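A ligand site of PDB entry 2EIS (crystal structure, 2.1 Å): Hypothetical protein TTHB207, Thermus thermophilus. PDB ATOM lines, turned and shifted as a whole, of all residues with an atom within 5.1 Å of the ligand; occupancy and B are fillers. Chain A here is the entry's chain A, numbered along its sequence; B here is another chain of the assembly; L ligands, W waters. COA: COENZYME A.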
ATOM      1  N   PHE A  35       8.862  10.580 -19.878  1.00  0.00           N
ATOM      2  CA  PHE A  35       8.563   9.302 -19.259  1.00  0.00           C
ATOM      3  C   PHE A  35       7.364   8.652 -19.943  1.00  0.00           C
ATOM      4  O   PHE A  35       7.354   7.455 -20.217  1.00  0.00           O
ATOM      5  CB  PHE A  35       8.302   9.513 -17.764  1.00  0.00           C
ATOM      6  CG  PHE A  35       7.956   8.241 -17.015  1.00  0.00           C
ATOM      7  CD1 PHE A  35       6.682   7.671 -17.131  1.00  0.00           C
ATOM      8  CD2 PHE A  35       8.883   7.628 -16.188  1.00  0.00           C
ATOM      9  CE1 PHE A  35       6.352   6.511 -16.434  1.00  0.00           C
ATOM     10  CE2 PHE A  35       8.570   6.462 -15.494  1.00  0.00           C
ATOM     11  CZ  PHE A  35       7.300   5.905 -15.605  1.00  0.00           C
ATOM     12  N   VAL A  47      12.875   4.150 -17.086  1.00  0.00           N
ATOM     13  CA  VAL A  47      13.442   5.038 -16.089  1.00  0.00           C
ATOM     14  C   VAL A  47      14.260   6.095 -16.815  1.00  0.00           C
ATOM     15  O   VAL A  47      14.732   5.865 -17.926  1.00  0.00           O
ATOM     16  CB  VAL A  47      14.382   4.299 -15.098  1.00  0.00           C
ATOM     17  CG1 VAL A  47      13.589   3.296 -14.267  1.00  0.00           C
ATOM     18  CG2 VAL A  47      15.508   3.588 -15.857  1.00  0.00           C
ATOM     19  N   THR A  48      14.399   7.263 -16.199  1.00  0.00           N
ATOM     20  CA  THR A  48      15.194   8.328 -16.799  1.00  0.00           C
ATOM     21  C   THR A  48      16.644   8.082 -16.379  1.00  0.00           C
ATOM     22  O   THR A  48      16.915   7.904 -15.188  1.00  0.00           O
ATOM     23  CB  THR A  48      14.778   9.710 -16.271  1.00  0.00           C
ATOM     24  OG1 THR A  48      13.416   9.989 -16.653  1.00  0.00           O
ATOM     25  CG2 THR A  48      15.688  10.783 -16.856  1.00  0.00           C
ATOM     26  N   VAL A  49      17.566   8.065 -17.327  1.00  0.00           N
ATOM     27  CA  VAL A  49      18.960   7.830 -16.985  1.00  0.00           C
ATOM     28  C   VAL A  49      19.810   9.050 -17.274  1.00  0.00           C
ATOM     29  O   VAL A  49      20.877   9.239 -16.682  1.00  0.00           O
ATOM     30  CB  VAL A  49      19.553   6.633 -17.762  1.00  0.00           C
ATOM     31  CG1 VAL A  49      19.678   6.961 -19.258  1.00  0.00           C
ATOM     32  CG2 VAL A  49      20.926   6.271 -17.198  1.00  0.00           C
ATOM     33  N   HIS A  50      19.317   9.903 -18.156  1.00  0.00           N
ATOM     34  CA  HIS A  50      20.092  11.049 -18.553  1.00  0.00           C
ATOM     35  C   HIS A  50      19.249  12.182 -19.105  1.00  0.00           C
ATOM     36  O   HIS A  50      18.201  11.954 -19.695  1.00  0.00           O
ATOM     37  CB  HIS A  50      21.093  10.603 -19.627  1.00  0.00           C
ATOM     38  CG  HIS A  50      22.056  11.662 -20.061  1.00  0.00           C
ATOM     39  ND1 HIS A  50      23.141  12.051 -19.302  1.00  0.00           N
ATOM     40  CD2 HIS A  50      22.118  12.394 -21.199  1.00  0.00           C
ATOM     41  CE1 HIS A  50      23.821  12.982 -19.944  1.00  0.00           C
ATOM     42  NE2 HIS A  50      23.226  13.203 -21.105  1.00  0.00           N
ATOM     43  N   GLY A  76      18.177   3.314 -29.342  1.00  0.00           N
ATOM     44  CA  GLY A  76      19.376   2.500 -29.370  1.00  0.00           C
ATOM     45  C   GLY A  76      18.925   1.054 -29.267  1.00  0.00           C
ATOM     46  O   GLY A  76      18.265   0.550 -30.173  1.00  0.00           O
ATOM     47  N   ARG A  77      19.267   0.404 -28.167  1.00  0.00           N
ATOM     48  CA  ARG A  77      18.832  -0.976 -27.960  1.00  0.00           C
ATOM     49  C   ARG A  77      17.759  -0.999 -26.871  1.00  0.00           C
ATOM     50  O   ARG A  77      16.645  -1.461 -27.087  1.00  0.00           O
ATOM     51  CB  ARG A  77      20.015  -1.869 -27.562  1.00  0.00           C
ATOM     52  CG  ARG A  77      19.584  -3.285 -27.206  1.00  0.00           C
ATOM     53  CD  ARG A  77      20.780  -4.219 -27.023  1.00  0.00           C
ATOM     54  NE  ARG A  77      20.671  -4.971 -25.773  1.00  0.00           N
ATOM     55  CZ  ARG A  77      21.043  -4.497 -24.582  1.00  0.00           C
ATOM     56  NH1 ARG A  77      21.540  -3.268 -24.477  1.00  0.00           N
ATOM     57  NH2 ARG A  77      20.888  -5.247 -23.498  1.00  0.00           N
ATOM     58  N   THR A  78      18.116  -0.509 -25.686  1.00  0.00           N
ATOM     59  CA  THR A  78      17.165  -0.463 -24.577  1.00  0.00           C
ATOM     60  C   THR A  78      16.872   0.999 -24.226  1.00  0.00           C
ATOM     61  O   THR A  78      15.961   1.276 -23.443  1.00  0.00           O
ATOM     62  CB  THR A  78      17.714  -1.160 -23.327  1.00  0.00           C
ATOM     63  OG1 THR A  78      18.830  -0.413 -22.814  1.00  0.00           O
ATOM     64  CG2 THR A  78      18.169  -2.586 -23.653  1.00  0.00           C
ATOM     65  N   SER A  79      17.646   1.913 -24.810  1.00  0.00           N
ATOM     66  CA  SER A  79      17.487   3.328 -24.527  1.00  0.00           C
ATOM     67  C   SER A  79      16.738   4.109 -25.602  1.00  0.00           C
ATOM     68  O   SER A  79      16.673   3.702 -26.761  1.00  0.00           O
ATOM     69  CB  SER A  79      18.872   3.973 -24.317  1.00  0.00           C
ATOM     70  OG  SER A  79      19.601   4.043 -25.532  1.00  0.00           O
ATOM     71  N   VAL A 106      17.073  10.911 -21.948  1.00  0.00           N
ATOM     72  CA  VAL A 106      17.324   9.542 -22.376  1.00  0.00           C
ATOM     73  C   VAL A 106      16.681   8.636 -21.339  1.00  0.00           C
ATOM     74  O   VAL A 106      16.965   8.729 -20.134  1.00  0.00           O
ATOM     75  CB  VAL A 106      18.844   9.212 -22.464  1.00  0.00           C
ATOM     76  CG1 VAL A 106      19.022   7.760 -22.919  1.00  0.00           C
ATOM     77  CG2 VAL A 106      19.534  10.172 -23.459  1.00  0.00           C
ATOM     78  N   VAL A 108      15.469   4.527 -20.331  1.00  0.00           N
ATOM     79  CA  VAL A 108      15.826   3.131 -20.543  1.00  0.00           C
ATOM     80  C   VAL A 108      14.712   2.187 -20.098  1.00  0.00           C
ATOM     81  O   VAL A 108      14.195   2.311 -18.981  1.00  0.00           O
ATOM     82  CB  VAL A 108      17.110   2.770 -19.731  1.00  0.00           C
ATOM     83  CG1 VAL A 108      17.440   1.299 -19.929  1.00  0.00           C
ATOM     84  CG2 VAL A 108      18.273   3.653 -20.170  1.00  0.00           C
ATOM     85  N   VAL A 110      13.229  -1.285 -18.783  1.00  0.00           N
ATOM     86  CA  VAL A 110      13.776  -2.328 -17.915  1.00  0.00           C
ATOM     87  C   VAL A 110      12.771  -3.437 -17.685  1.00  0.00           C
ATOM     88  O   VAL A 110      11.563  -3.229 -17.803  1.00  0.00           O
ATOM     89  CB  VAL A 110      14.183  -1.748 -16.533  1.00  0.00           C
ATOM     90  CG1 VAL A 110      15.228  -0.637 -16.705  1.00  0.00           C
ATOM     91  CG2 VAL A 110      12.949  -1.211 -15.806  1.00  0.00           C
ATOM     92  N   GLY A 114      14.390  -5.107 -13.229  1.00  0.00           N
ATOM     93  CA  GLY A 114      15.026  -3.797 -13.239  1.00  0.00           C
ATOM     94  C   GLY A 114      16.219  -3.709 -14.176  1.00  0.00           C
ATOM     95  O   GLY A 114      16.979  -2.741 -14.142  1.00  0.00           O
ATOM     96  N   PRO A 116      17.996  -3.424 -17.961  1.00  0.00           N
ATOM     97  CA  PRO A 116      17.729  -2.830 -19.277  1.00  0.00           C
ATOM     98  C   PRO A 116      17.131  -3.860 -20.228  1.00  0.00           C
ATOM     99  O   PRO A 116      17.657  -4.963 -20.362  1.00  0.00           O
ATOM    100  CB  PRO A 116      19.106  -2.353 -19.716  1.00  0.00           C
ATOM    101  CG  PRO A 116      19.697  -1.889 -18.417  1.00  0.00           C
ATOM    102  CD  PRO A 116      19.316  -3.011 -17.463  1.00  0.00           C
ATOM    103  N   ASN B  16       7.858   7.271  -7.694  1.00  0.00           N
ATOM    104  CA  ASN B  16       7.133   6.880  -8.892  1.00  0.00           C
ATOM    105  C   ASN B  16       6.447   5.588  -8.448  1.00  0.00           C
ATOM    106  O   ASN B  16       6.582   5.171  -7.298  1.00  0.00           O
ATOM    107  CB  ASN B  16       8.103   6.572 -10.021  1.00  0.00           C
ATOM    108  CG  ASN B  16       9.246   5.682  -9.574  1.00  0.00           C
ATOM    109  OD1 ASN B  16       9.029   4.691  -8.882  1.00  0.00           O
ATOM    110  ND2 ASN B  16      10.464   6.026  -9.976  1.00  0.00           N
ATOM    111  N   THR B  20      10.706   4.211  -6.078  1.00  0.00           N
ATOM    112  CA  THR B  20      11.983   4.892  -6.062  1.00  0.00           C
ATOM    113  C   THR B  20      11.709   6.366  -6.317  1.00  0.00           C
ATOM    114  O   THR B  20      10.647   6.727  -6.841  1.00  0.00           O
ATOM    115  CB  THR B  20      12.956   4.380  -7.145  1.00  0.00           C
ATOM    116  OG1 THR B  20      12.361   4.503  -8.445  1.00  0.00           O
ATOM    117  CG2 THR B  20      13.300   2.914  -6.897  1.00  0.00           C
ATOM    118  N   LEU B  21      12.645   7.217  -5.923  1.00  0.00           N
ATOM    119  CA  LEU B  21      12.495   8.661  -6.094  1.00  0.00           C
ATOM    120  C   LEU B  21      12.298   8.998  -7.556  1.00  0.00           C
ATOM    121  O   LEU B  21      13.130   8.632  -8.408  1.00  0.00           O
ATOM    122  CB  LEU B  21      13.733   9.368  -5.532  1.00  0.00           C
ATOM    123  CG  LEU B  21      13.772  10.896  -5.537  1.00  0.00           C
ATOM    124  CD1 LEU B  21      12.615  11.438  -4.708  1.00  0.00           C
ATOM    125  CD2 LEU B  21      15.117  11.364  -4.979  1.00  0.00           C
ATOM    126  N   PHE B  22      11.214   9.698  -7.859  1.00  0.00           N
ATOM    127  CA  PHE B  22      10.884  10.083  -9.239  1.00  0.00           C
ATOM    128  C   PHE B  22      11.935  11.033  -9.804  1.00  0.00           C
ATOM    129  O   PHE B  22      12.345  12.000  -9.152  1.00  0.00           O
ATOM    130  CB  PHE B  22       9.499  10.753  -9.305  1.00  0.00           C
ATOM    131  CG  PHE B  22       9.142  11.295 -10.671  1.00  0.00           C
ATOM    132  CD1 PHE B  22       8.665  12.601 -10.817  1.00  0.00           C
ATOM    133  CD2 PHE B  22       9.296  10.513 -11.814  1.00  0.00           C
ATOM    134  CE1 PHE B  22       8.356  13.118 -12.080  1.00  0.00           C
ATOM    135  CE2 PHE B  22       8.983  11.017 -13.082  1.00  0.00           C
ATOM    136  CZ  PHE B  22       8.514  12.320 -13.208  1.00  0.00           C
ATOM    137  N   GLY B  23      12.351  10.778 -11.046  1.00  0.00           N
ATOM    138  CA  GLY B  23      13.362  11.607 -11.676  1.00  0.00           C
ATOM    139  C   GLY B  23      13.016  13.086 -11.751  1.00  0.00           C
ATOM    140  O   GLY B  23      13.888  13.934 -11.599  1.00  0.00           O
ATOM    141  N   ASP B  55      23.011  12.927 -14.962  1.00  0.00           N
ATOM    142  CA  ASP B  55      23.020  11.474 -15.048  1.00  0.00           C
ATOM    143  C   ASP B  55      22.373  10.859 -13.807  1.00  0.00           C
ATOM    144  O   ASP B  55      22.639  11.279 -12.684  1.00  0.00           O
ATOM    145  CB  ASP B  55      24.459  10.965 -15.178  1.00  0.00           C
ATOM    146  CG  ASP B  55      25.114  11.399 -16.477  1.00  0.00           C
ATOM    147  OD1 ASP B  55      26.173  12.061 -16.414  1.00  0.00           O
ATOM    148  OD2 ASP B  55      24.566  11.090 -17.557  1.00  0.00           O
ATOM    149  N   PHE B  56      21.521   9.875 -14.040  1.00  0.00           N
ATOM    150  CA  PHE B  56      20.839   9.162 -12.969  1.00  0.00           C
ATOM    151  C   PHE B  56      21.540   7.800 -12.970  1.00  0.00           C
ATOM    152  O   PHE B  56      21.162   6.894 -13.708  1.00  0.00           O
ATOM    153  CB  PHE B  56      19.350   9.010 -13.296  1.00  0.00           C
ATOM    154  CG  PHE B  56      18.612  10.319 -13.390  1.00  0.00           C
ATOM    155  CD1 PHE B  56      17.959  10.847 -12.278  1.00  0.00           C
ATOM    156  CD2 PHE B  56      18.596  11.035 -14.577  1.00  0.00           C
ATOM    157  CE1 PHE B  56      17.293  12.086 -12.361  1.00  0.00           C
ATOM    158  CE2 PHE B  56      17.941  12.273 -14.669  1.00  0.00           C
ATOM    159  CZ  PHE B  56      17.285  12.791 -13.549  1.00  0.00           C
ATOM    160  N   LYS B  57      22.558   7.687 -12.136  1.00  0.00           N
ATOM    161  CA  LYS B  57      23.370   6.481 -12.047  1.00  0.00           C
ATOM    162  C   LYS B  57      22.752   5.329 -11.286  1.00  0.00           C
ATOM    163  O   LYS B  57      22.795   4.184 -11.742  1.00  0.00           O
ATOM    164  CB  LYS B  57      24.722   6.820 -11.408  1.00  0.00           C
ATOM    165  CG  LYS B  57      25.460   7.966 -12.081  1.00  0.00           C
ATOM    166  CD  LYS B  57      25.922   7.596 -13.482  1.00  0.00           C
ATOM    167  CE  LYS B  57      26.757   8.719 -14.104  1.00  0.00           C
ATOM    168  NZ  LYS B  57      27.161   8.421 -15.512  1.00  0.00           N
ATOM    169  N   ARG B  58      22.190   5.623 -10.132  1.00  0.00           N
ATOM    170  CA  ARG B  58      21.591   4.584  -9.310  1.00  0.00           C
ATOM    171  C   ARG B  58      20.229   5.032  -8.787  1.00  0.00           C
ATOM    172  O   ARG B  58      20.004   6.217  -8.550  1.00  0.00           O
ATOM    173  CB  ARG B  58      22.542   4.237  -8.159  1.00  0.00           C
ATOM    174  CG  ARG B  58      23.798   3.454  -8.606  1.00  0.00           C
ATOM    175  CD  ARG B  58      24.896   3.483  -7.551  1.00  0.00           C
ATOM    176  NE  ARG B  58      25.700   4.702  -7.630  1.00  0.00           N
ATOM    177  CZ  ARG B  58      26.752   4.856  -8.420  1.00  0.00           C
ATOM    178  NH1 ARG B  58      27.148   3.873  -9.211  1.00  0.00           N
ATOM    179  NH2 ARG B  58      27.407   6.021  -8.443  1.00  0.00           N
ATOM    180  N   PRO B  59      19.297   4.081  -8.597  1.00  0.00           N
ATOM    181  CA  PRO B  59      17.960   4.423  -8.095  1.00  0.00           C
ATOM    182  C   PRO B  59      17.991   4.772  -6.610  1.00  0.00           C
ATOM    183  O   PRO B  59      18.879   4.327  -5.871  1.00  0.00           O
ATOM    184  CB  PRO B  59      17.151   3.168  -8.372  1.00  0.00           C
ATOM    185  CG  PRO B  59      18.171   2.079  -8.182  1.00  0.00           C
ATOM    186  CD  PRO B  59      19.410   2.629  -8.867  1.00  0.00           C
ATOM    187  N   VAL B  60      17.038   5.595  -6.178  1.00  0.00           N
ATOM    188  CA  VAL B  60      16.939   5.978  -4.784  1.00  0.00           C
ATOM    189  C   VAL B  60      15.664   5.347  -4.227  1.00  0.00           C
ATOM    190  O   VAL B  60      14.566   5.776  -4.544  1.00  0.00           O
ATOM    191  CB  VAL B  60      16.866   7.506  -4.624  1.00  0.00           C
ATOM    192  CG1 VAL B  60      16.823   7.879  -3.152  1.00  0.00           C
ATOM    193  CG2 VAL B  60      18.061   8.166  -5.301  1.00  0.00           C
HETATM  194  N1A COA L   1      23.666   8.672 -20.530  1.00  0.00           N
HETATM  195  C2A COA L   1      23.057   8.156 -21.616  1.00  0.00           C
HETATM  196  N3A COA L   1      22.655   6.886 -21.826  1.00  0.00           N
HETATM  197  C4A COA L   1      22.999   6.094 -20.795  1.00  0.00           C
HETATM  198  C5A COA L   1      23.613   6.489 -19.607  1.00  0.00           C
HETATM  199  C6A COA L   1      23.892   7.861 -19.461  1.00  0.00           C
HETATM  200  N6A COA L   1      24.251   8.424 -18.300  1.00  0.00           N
HETATM  201  N7A COA L   1      23.800   5.397 -18.771  1.00  0.00           N
HETATM  202  C8A COA L   1      23.261   4.393 -19.432  1.00  0.00           C
HETATM  203  N9A COA L   1      22.815   4.739 -20.686  1.00  0.00           N
HETATM  204  C1B COA L   1      22.202   3.860 -21.682  1.00  0.00           C
HETATM  205  C2B COA L   1      23.204   2.936 -22.371  1.00  0.00           C
HETATM  206  O2B COA L   1      23.827   3.602 -23.454  1.00  0.00           O
HETATM  207  C3B COA L   1      22.290   1.807 -22.813  1.00  0.00           C
HETATM  208  O3B COA L   1      21.588   2.196 -23.976  1.00  0.00           O
HETATM  209  P3B COA L   1      21.421   1.155 -25.182  1.00  0.00           P
HETATM  210  O7A COA L   1      20.514   1.741 -26.204  1.00  0.00           O
HETATM  211  O8A COA L   1      20.939  -0.149 -24.694  1.00  0.00           O
HETATM  212  O9A COA L   1      22.749   0.914 -25.812  1.00  0.00           O
HETATM  213  C4B COA L   1      21.309   1.694 -21.642  1.00  0.00           C
HETATM  214  O4B COA L   1      21.298   3.006 -21.025  1.00  0.00           O
HETATM  215  C5B COA L   1      21.633   0.645 -20.611  1.00  0.00           C
HETATM  216  O5B COA L   1      23.015   0.714 -20.255  1.00  0.00           O
HETATM  217  P1A COA L   1      23.675  -0.403 -19.325  1.00  0.00           P
HETATM  218  O1A COA L   1      25.127  -0.107 -19.249  1.00  0.00           O
HETATM  219  O2A COA L   1      23.223  -1.736 -19.801  1.00  0.00           O
HETATM  220  O3A COA L   1      23.006  -0.159 -17.900  1.00  0.00           O
HETATM  221  P2A COA L   1      23.692   0.767 -16.785  1.00  0.00           P
HETATM  222  O4A COA L   1      24.654  -0.061 -16.017  1.00  0.00           O
HETATM  223  O5A COA L   1      24.158   2.023 -17.424  1.00  0.00           O
HETATM  224  O6A COA L   1      22.473   1.116 -15.834  1.00  0.00           O
HETATM  225  CBP COA L   1      20.270   1.949 -15.241  1.00  0.00           C
HETATM  226  CCP COA L   1      21.265   1.677 -16.365  1.00  0.00           C
HETATM  227  CDP COA L   1      19.118   2.796 -15.797  1.00  0.00           C
HETATM  228  CEP COA L   1      19.741   0.608 -14.740  1.00  0.00           C
HETATM  229  CAP COA L   1      20.979   2.704 -14.101  1.00  0.00           C
HETATM  230  OAP COA L   1      21.696   3.824 -14.643  1.00  0.00           O
HETATM  231  C9P COA L   1      19.943   3.205 -13.093  1.00  0.00           C
HETATM  232  O9P COA L   1      19.297   2.408 -12.415  1.00  0.00           O
HETATM  233  N8P COA L   1      19.837   4.519 -12.951  1.00  0.00           N
HETATM  234  C7P COA L   1      18.855   5.170 -12.072  1.00  0.00           C
HETATM  235  C6P COA L   1      17.514   5.396 -12.769  1.00  0.00           C
HETATM  236  C5P COA L   1      16.549   6.214 -11.922  1.00  0.00           C
HETATM  237  O5P COA L   1      16.416   5.973 -10.725  1.00  0.00           O
HETATM  238  N4P COA L   1      15.990   7.272 -12.508  1.00  0.00           N
HETATM  239  C3P COA L   1      15.149   8.232 -11.794  1.00  0.00           C
HETATM  240  C2P COA L   1      13.788   7.653 -11.496  1.00  0.00           C
HETATM  241  S1P COA L   1      12.671   7.649 -12.927  1.00  0.00           S
HETATM  242  O   HOH W   1      16.526   2.209 -12.055  1.00  0.00           O
HETATM  243  O   HOH W   2      23.131   2.258 -28.161  1.00  0.00           O
HETATM  244  O   HOH W   3      26.347  10.709 -20.766  1.00  0.00           O
HETATM  245  O   HOH W   4      14.570   3.831 -10.304  1.00  0.00           O
HETATM  246  O   HOH W   5      15.435   7.012  -8.311  1.00  0.00           O
HETATM  247  O   HOH W   6      22.370  -3.183 -22.159  1.00  0.00           O
HETATM  248  O   HOH W   7      24.029   4.435 -15.897  1.00  0.00           O
HETATM  249  O   HOH W   8      21.935  -4.072 -19.178  1.00  0.00           O
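N of Gly 23 of chain B lies close to S1P of the ligand, 3.7 Å away. N of Thr 48 lies close to S1P of the ligand, at 3.7 Å. The backbone carbonyl oxygen (O) of Thr 48 sits at hydrogen-bond distance from a nitrogen (N4P) of the ligand (2.9 Å). The backbone NH (N) of Thr 78 lies within hydrogen-bond range of an oxygen (O8A) of the ligand. The backbone NH (N) of Arg 77 lies within hydrogen-bond range of an oxygen (O7A) of the ligand, 2.7 Å away. The backbone carbonyl oxygen of Lys 57 of chain B lies within hydrogen-bond range of an oxygen (OAP) of the ligand, 3.1 Å away. An oxygen (O7A) of the ligand lies within hydrogen-bond range of the side-chain hydroxyl (OG) of Ser 79 (2.6 Å). A nitrogen (N6A) of the ligand sits at hydrogen-bond distance from the side-chain carboxylate (OD2) of Asp 55 of chain B. N of Ser 79 lies within hydrogen-bond range of O7A of the ligand. The side-chain hydroxyl of Thr 78 lies within hydrogen-bond range of an oxygen (O8A) of the ligand (2.8 Å). The backbone carbonyl oxygen (O) of Phe 56 of chain B lies within hydrogen-bond range of a nitrogen (N8P) of the ligand (2.8 Å). The guanidinium group of Arg 77 lies within salt-bridge range of an oxygen (O8A) of the ligand.
N of Phe 56 of chain B lies within hydrogen-bond range of O of Val 49 (2.8 Å). The side-chain carboxylate (OD1) of Asp 55 of chain B lies within salt-bridge range of the side-chain amino group (NZ) of Lys 57 of chain B (3.9 Å). OD2 of Asp 55 of chain B is in hydrogen-bond range of ND1 of His 50, at 2.4 Å. The backbone carbonyl oxygen (O) of Val 106 lies within hydrogen-bond range of the backbone NH (N) of Val 49 (2.9 Å). N of Val 106 is in hydrogen-bond range of O of His 50, 2.7 Å away. N of Val 108 lies within hydrogen-bond range of O of Val 47.
Val 47 touches the ligand (CG2 to CDP, 3.7 Å). Val 49 touches the ligand. His 50 touches the ligand. CA of Gly 76 touches O7A of the ligand, 3.4 Å away. CG1 of Val 106 touches N3A of the ligand, 3.9 Å away. CG2 of Val 108 touches O4B of the ligand (3.2 Å). CG of Pro 116 touches O3A of the ligand, at 3.8 Å. O of Leu 21 of chain B touches C2P of the ligand, 3.3 Å away. C of Arg 58 of chain B touches C7P of the ligand, at 3.6 Å. Pro 59 of chain B touches the ligand. Hydrophobic or aromatic side chains within 4 Å of the ligand: Val 47, Val 49, His 50, Val 106, Val 108, Pro 116, Phe 56 of chain B and Pro 59 of chain B. 18 residues have an atom within 4 Å of the ligand: Val 47, Thr 48, Val 49, His 50, Gly 76, Arg 77, Thr 78, Ser 79, Val 106, Val 108, Pro 116, Leu 21 of chain B, Gly 23 of chain B, Asp 55 of chain B, Phe 56 of chain B, Lys 57 of chain B, Arg 58 of chain B and Pro 59 of chain B.
Water W5 lies within hydrogen-bond range of an oxygen (O5P) of the ligand (2.8 Å) and the backbone carbonyl oxygen (O) of Leu 21 of chain B (2.8 Å). Water W4 bridges O5P of the ligand (2.9 Å) and OG1 of Thr 20 of chain B (3.0 Å). Water W6 bridges NH1 of Arg 77 (2.5 Å) and O2A of the ligand (2.9 Å).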
